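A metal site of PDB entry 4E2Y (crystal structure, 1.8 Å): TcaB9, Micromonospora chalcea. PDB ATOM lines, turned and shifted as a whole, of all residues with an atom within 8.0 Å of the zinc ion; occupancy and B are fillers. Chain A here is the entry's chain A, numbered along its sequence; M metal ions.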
ATOM      1  N   ALA A  14      18.430   0.244   3.731  1.00  0.00           N
ATOM      2  CA  ALA A  14      17.137   0.178   4.438  1.00  0.00           C
ATOM      3  C   ALA A  14      16.436   1.531   4.358  1.00  0.00           C
ATOM      4  O   ALA A  14      17.087   2.548   4.594  1.00  0.00           O
ATOM      5  CB  ALA A  14      17.258  -0.185   5.921  1.00  0.00           C
ATOM      6  N   CYS A  15      15.148   1.523   4.059  1.00  0.00           N
ATOM      7  CA  CYS A  15      14.264   2.683   4.111  1.00  0.00           C
ATOM      8  C   CYS A  15      14.352   3.423   5.458  1.00  0.00           C
ATOM      9  O   CYS A  15      14.245   2.820   6.538  1.00  0.00           O
ATOM     10  CB  CYS A  15      12.821   2.250   3.859  1.00  0.00           C
ATOM     11  SG  CYS A  15      11.705   3.672   3.820  1.00  0.00           S
ATOM     12  N   ARG A  16      14.598   4.729   5.359  1.00  0.00           N
ATOM     13  CA  ARG A  16      14.605   5.624   6.497  1.00  0.00           C
ATOM     14  C   ARG A  16      13.265   5.816   7.186  1.00  0.00           C
ATOM     15  O   ARG A  16      13.245   6.231   8.349  1.00  0.00           O
ATOM     16  CB  ARG A  16      15.293   6.954   6.152  1.00  0.00           C
ATOM     17  CG  ARG A  16      16.805   6.763   6.136  1.00  0.00           C
ATOM     18  CD  ARG A  16      17.278   6.402   7.572  1.00  0.00           C
ATOM     19  NE  ARG A  16      18.314   7.333   8.012  1.00  0.00           N
ATOM     20  CZ  ARG A  16      18.441   7.874   9.213  1.00  0.00           C
ATOM     21  NH1 ARG A  16      17.605   7.627  10.216  1.00  0.00           N
ATOM     22  NH2 ARG A  16      19.482   8.681   9.386  1.00  0.00           N
ATOM     23  N   VAL A  17      12.181   5.444   6.505  1.00  0.00           N
ATOM     24  CA  VAL A  17      10.855   5.653   7.091  1.00  0.00           C
ATOM     25  C   VAL A  17      10.397   4.368   7.779  1.00  0.00           C
ATOM     26  O   VAL A  17      10.000   4.344   8.949  1.00  0.00           O
ATOM     27  CB  VAL A  17       9.820   6.081   6.032  1.00  0.00           C
ATOM     28  CG1 VAL A  17       8.408   6.049   6.605  1.00  0.00           C
ATOM     29  CG2 VAL A  17      10.147   7.505   5.589  1.00  0.00           C
ATOM     30  N   CYS A  18      10.485   3.280   7.026  1.00  0.00           N
ATOM     31  CA  CYS A  18       9.932   2.029   7.551  1.00  0.00           C
ATOM     32  C   CYS A  18      10.901   0.846   7.705  1.00  0.00           C
ATOM     33  O   CYS A  18      10.443  -0.197   8.171  1.00  0.00           O
ATOM     34  CB  CYS A  18       8.751   1.581   6.691  1.00  0.00           C
ATOM     35  SG  CYS A  18       9.228   0.835   5.145  1.00  0.00           S
ATOM     36  N   GLY A  19      12.175   0.975   7.336  1.00  0.00           N
ATOM     37  CA  GLY A  19      13.081  -0.183   7.403  1.00  0.00           C
ATOM     38  C   GLY A  19      12.974  -1.187   6.261  1.00  0.00           C
ATOM     39  O   GLY A  19      13.743  -2.150   6.187  1.00  0.00           O
ATOM     40  N   GLY A  20      12.055  -0.963   5.343  1.00  0.00           N
ATOM     41  CA  GLY A  20      11.938  -1.787   4.156  1.00  0.00           C
ATOM     42  C   GLY A  20      13.112  -1.733   3.187  1.00  0.00           C
ATOM     43  O   GLY A  20      14.025  -0.931   3.358  1.00  0.00           O
ATOM     44  N   GLY A  21      13.107  -2.517   2.116  1.00  0.00           N
ATOM     45  CA  GLY A  21      14.201  -2.430   1.132  1.00  0.00           C
ATOM     46  C   GLY A  21      14.107  -1.404   0.019  1.00  0.00           C
ATOM     47  O   GLY A  21      13.089  -1.309  -0.677  1.00  0.00           O
ATOM     48  N   VAL A  22      15.179  -0.641  -0.174  1.00  0.00           N
ATOM     49  CA  VAL A  22      15.199   0.433  -1.183  1.00  0.00           C
ATOM     50  C   VAL A  22      15.835  -0.128  -2.447  1.00  0.00           C
ATOM     51  O   VAL A  22      16.972  -0.633  -2.422  1.00  0.00           O
ATOM     52  CB  VAL A  22      15.949   1.660  -0.622  1.00  0.00           C
ATOM     53  CG1 VAL A  22      16.206   2.713  -1.680  1.00  0.00           C
ATOM     54  CG2 VAL A  22      15.185   2.290   0.557  1.00  0.00           C
ATOM     55  N   ARG A  55      13.579   3.435  -4.450  1.00  0.00           N
ATOM     56  CA  ARG A  55      12.237   3.434  -3.881  1.00  0.00           C
ATOM     57  C   ARG A  55      12.132   2.282  -2.879  1.00  0.00           C
ATOM     58  O   ARG A  55      12.479   1.143  -3.207  1.00  0.00           O
ATOM     59  CB  ARG A  55      11.197   3.271  -4.985  1.00  0.00           C
ATOM     60  CG  ARG A  55       9.776   3.574  -4.537  1.00  0.00           C
ATOM     61  CD  ARG A  55       8.702   2.812  -5.308  1.00  0.00           C
ATOM     62  NE  ARG A  55       8.821   1.365  -5.110  1.00  0.00           N
ATOM     63  CZ  ARG A  55       8.034   0.431  -5.652  1.00  0.00           C
ATOM     64  NH1 ARG A  55       8.264  -0.842  -5.350  1.00  0.00           N
ATOM     65  NH2 ARG A  55       7.047   0.737  -6.475  1.00  0.00           N
ATOM     66  N   CYS A  56      11.680   2.609  -1.681  1.00  0.00           N
ATOM     67  CA  CYS A  56      11.290   1.566  -0.740  1.00  0.00           C
ATOM     68  C   CYS A  56      10.207   0.633  -1.295  1.00  0.00           C
ATOM     69  O   CYS A  56       9.205   1.088  -1.839  1.00  0.00           O
ATOM     70  CB  CYS A  56      10.807   2.177   0.580  1.00  0.00           C
ATOM     71  SG  CYS A  56      10.322   0.924   1.821  1.00  0.00           S
ATOM     72  N   ASP A  57      10.409  -0.662  -1.099  1.00  0.00           N
ATOM     73  CA  ASP A  57       9.452  -1.705  -1.478  1.00  0.00           C
ATOM     74  C   ASP A  57       8.156  -1.754  -0.682  1.00  0.00           C
ATOM     75  O   ASP A  57       7.135  -2.261  -1.163  1.00  0.00           O
ATOM     76  CB  ASP A  57      10.129  -3.073  -1.362  1.00  0.00           C
ATOM     77  CG  ASP A  57      11.120  -3.253  -2.473  1.00  0.00           C
ATOM     78  OD1 ASP A  57      10.872  -2.517  -3.443  1.00  0.00           O
ATOM     79  OD2 ASP A  57      12.080  -4.034  -2.360  1.00  0.00           O
ATOM     80  N   SER A  58       8.187  -1.265   0.546  1.00  0.00           N
ATOM     81  CA  SER A  58       7.032  -1.363   1.423  1.00  0.00           C
ATOM     82  C   SER A  58       6.155  -0.125   1.413  1.00  0.00           C
ATOM     83  O   SER A  58       4.924  -0.207   1.328  1.00  0.00           O
ATOM     84  CB  SER A  58       7.467  -1.550   2.880  1.00  0.00           C
ATOM     85  OG  SER A  58       8.223  -2.743   2.941  1.00  0.00           O
ATOM     86  N   CYS A  59       6.814   1.028   1.536  1.00  0.00           N
ATOM     87  CA  CYS A  59       6.092   2.274   1.777  1.00  0.00           C
ATOM     88  C   CYS A  59       6.129   3.252   0.607  1.00  0.00           C
ATOM     89  O   CYS A  59       5.452   4.296   0.636  1.00  0.00           O
ATOM     90  CB  CYS A  59       6.627   2.912   3.056  1.00  0.00           C
ATOM     91  SG  CYS A  59       8.139   3.865   2.817  1.00  0.00           S
ATOM     92  N   GLU A  60       6.862   2.849  -0.427  1.00  0.00           N
ATOM     93  CA  GLU A  60       6.970   3.619  -1.669  1.00  0.00           C
ATOM     94  C   GLU A  60       7.703   4.970  -1.630  1.00  0.00           C
ATOM     95  O   GLU A  60       7.637   5.745  -2.602  1.00  0.00           O
ATOM     96  CB  GLU A  60       5.624   3.748  -2.401  1.00  0.00           C
ATOM     97  CG  GLU A  60       5.149   2.378  -2.888  1.00  0.00           C
ATOM     98  CD  GLU A  60       3.893   2.574  -3.714  1.00  0.00           C
ATOM     99  OE1 GLU A  60       3.970   3.118  -4.822  1.00  0.00           O
ATOM    100  OE2 GLU A  60       2.803   2.250  -3.211  1.00  0.00           O
ATOM    101  N   MET A  61       8.346   5.218  -0.506  1.00  0.00           N
ATOM    102  CA  MET A  61       9.214   6.390  -0.285  1.00  0.00           C
ATOM    103  C   MET A  61      10.413   6.370  -1.225  1.00  0.00           C
ATOM    104  O   MET A  61      11.273   5.470  -1.225  1.00  0.00           O
ATOM    105  CB  MET A  61       9.716   6.501   1.171  1.00  0.00           C
ATOM    106  CG  MET A  61      10.411   7.845   1.474  1.00  0.00           C
ATOM    107  SD  MET A  61       9.442   9.343   1.065  1.00  0.00           S
ATOM    108  CE  MET A  61       8.430   9.402   2.554  1.00  0.00           C
ATOM    109  N   VAL A  62      10.479   7.411  -2.040  1.00  0.00           N
ATOM    110  CA  VAL A  62      11.646   7.624  -2.927  1.00  0.00           C
ATOM    111  C   VAL A  62      12.695   8.423  -2.158  1.00  0.00           C
ATOM    112  O   VAL A  62      12.424   9.454  -1.550  1.00  0.00           O
ATOM    113  CB  VAL A  62      11.224   8.319  -4.226  1.00  0.00           C
ATOM    114  CG1 VAL A  62      12.447   8.738  -5.027  1.00  0.00           C
ATOM    115  CG2 VAL A  62      10.321   7.342  -5.039  1.00  0.00           C
ATOM    116  N   GLN A  63      13.926   7.904  -2.196  1.00  0.00           N
ATOM    117  CA  GLN A  63      14.996   8.423  -1.335  1.00  0.00           C
ATOM    118  C   GLN A  63      16.381   8.094  -1.861  1.00  0.00           C
ATOM    119  O   GLN A  63      16.568   7.130  -2.619  1.00  0.00           O
ATOM    120  CB  GLN A  63      14.868   7.855   0.091  1.00  0.00           C
ATOM    121  CG  GLN A  63      15.044   6.330   0.202  1.00  0.00           C
ATOM    122  CD  GLN A  63      14.377   5.746   1.431  1.00  0.00           C
ATOM    123  OE1 GLN A  63      14.982   5.673   2.533  1.00  0.00           O
ATOM    124  NE2 GLN A  63      13.100   5.389   1.266  1.00  0.00           N
ATOM    125  N   PHE A 229      14.758  12.966   0.299  1.00  0.00           N
ATOM    126  CA  PHE A 229      13.456  12.399  -0.047  1.00  0.00           C
ATOM    127  C   PHE A 229      12.845  13.177  -1.207  1.00  0.00           C
ATOM    128  O   PHE A 229      12.933  14.407  -1.230  1.00  0.00           O
ATOM    129  CB  PHE A 229      12.480  12.494   1.136  1.00  0.00           C
ATOM    130  CG  PHE A 229      12.868  11.623   2.303  1.00  0.00           C
ATOM    131  CD1 PHE A 229      12.916  10.252   2.163  1.00  0.00           C
ATOM    132  CD2 PHE A 229      13.190  12.193   3.539  1.00  0.00           C
ATOM    133  CE1 PHE A 229      13.259   9.423   3.247  1.00  0.00           C
ATOM    134  CE2 PHE A 229      13.596  11.388   4.599  1.00  0.00           C
ATOM    135  CZ  PHE A 229      13.612  10.013   4.467  1.00  0.00           C
ATOM    136  N   SER A 235       3.568   8.327  -0.557  1.00  0.00           N
ATOM    137  CA  SER A 235       4.572   7.974   0.463  1.00  0.00           C
ATOM    138  C   SER A 235       4.395   8.809   1.722  1.00  0.00           C
ATOM    139  O   SER A 235       4.639   8.306   2.822  1.00  0.00           O
ATOM    140  CB  SER A 235       5.985   8.124  -0.112  1.00  0.00           C
ATOM    141  OG  SER A 235       6.261   9.469  -0.477  1.00  0.00           O
ATOM    142  N   MET A 239       3.917   7.339   5.549  1.00  0.00           N
ATOM    143  CA  MET A 239       4.777   7.801   6.657  1.00  0.00           C
ATOM    144  C   MET A 239       4.038   8.415   7.841  1.00  0.00           C
ATOM    145  O   MET A 239       4.397   8.256   9.014  1.00  0.00           O
ATOM    146  CB  MET A 239       5.757   8.869   6.122  1.00  0.00           C
ATOM    147  CG  MET A 239       6.587   9.642   7.137  1.00  0.00           C
ATOM    148  SD  MET A 239       7.755  10.787   6.264  1.00  0.00           S
ATOM    149  CE  MET A 239       6.659  12.146   5.864  1.00  0.00           C
ATOM    150  N   ARG A 242       2.114   5.712   9.737  1.00  0.00           N
ATOM    151  CA  ARG A 242       3.021   4.823  10.456  1.00  0.00           C
ATOM    152  C   ARG A 242       3.475   5.435  11.770  1.00  0.00           C
ATOM    153  O   ARG A 242       3.962   4.684  12.630  1.00  0.00           O
ATOM    154  CB  ARG A 242       4.211   4.422   9.573  1.00  0.00           C
ATOM    155  CG  ARG A 242       3.955   3.332   8.536  1.00  0.00           C
ATOM    156  CD  ARG A 242       5.146   3.226   7.599  1.00  0.00           C
ATOM    157  NE  ARG A 242       5.148   1.993   6.802  1.00  0.00           N
ATOM    158  CZ  ARG A 242       4.526   1.790   5.648  1.00  0.00           C
ATOM    159  NH1 ARG A 242       4.666   0.607   5.049  1.00  0.00           N
ATOM    160  NH2 ARG A 242       3.793   2.724   5.066  1.00  0.00           N
HETATM  161 ZN    ZN M   1       9.764   2.422   3.522  1.00  0.00          ZN
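The zinc ion is bound by the side-chain sulfur of Cys 59 (2.3 Å), the side-chain sulfur of Cys 15 (2.3 Å), the side-chain sulfur of Cys 18 (2.3 Å) and the side-chain sulfur of Cys 56 (2.3 Å).
N of Met 61 sits close to SG of Cys 59, 3.6 Å away. SG of Cys 15 sits close to N of Val 17 (3.3 Å). N of Cys 15 lies within hydrogen-bond range of O of Gly 20, 2.8 Å away. The side-chain sulfur of Cys 15 sits close to the side-chain amide nitrogen of Gln 63 (3.4 Å). SG of Cys 18 sits close to N of Gly 20, at 3.4 Å. The backbone NH of Ser 58 sits close to the side-chain sulfur of Cys 56 (3.3 Å). O of Met 61 sits at hydrogen-bond distance from N of Cys 56 (2.9 Å).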
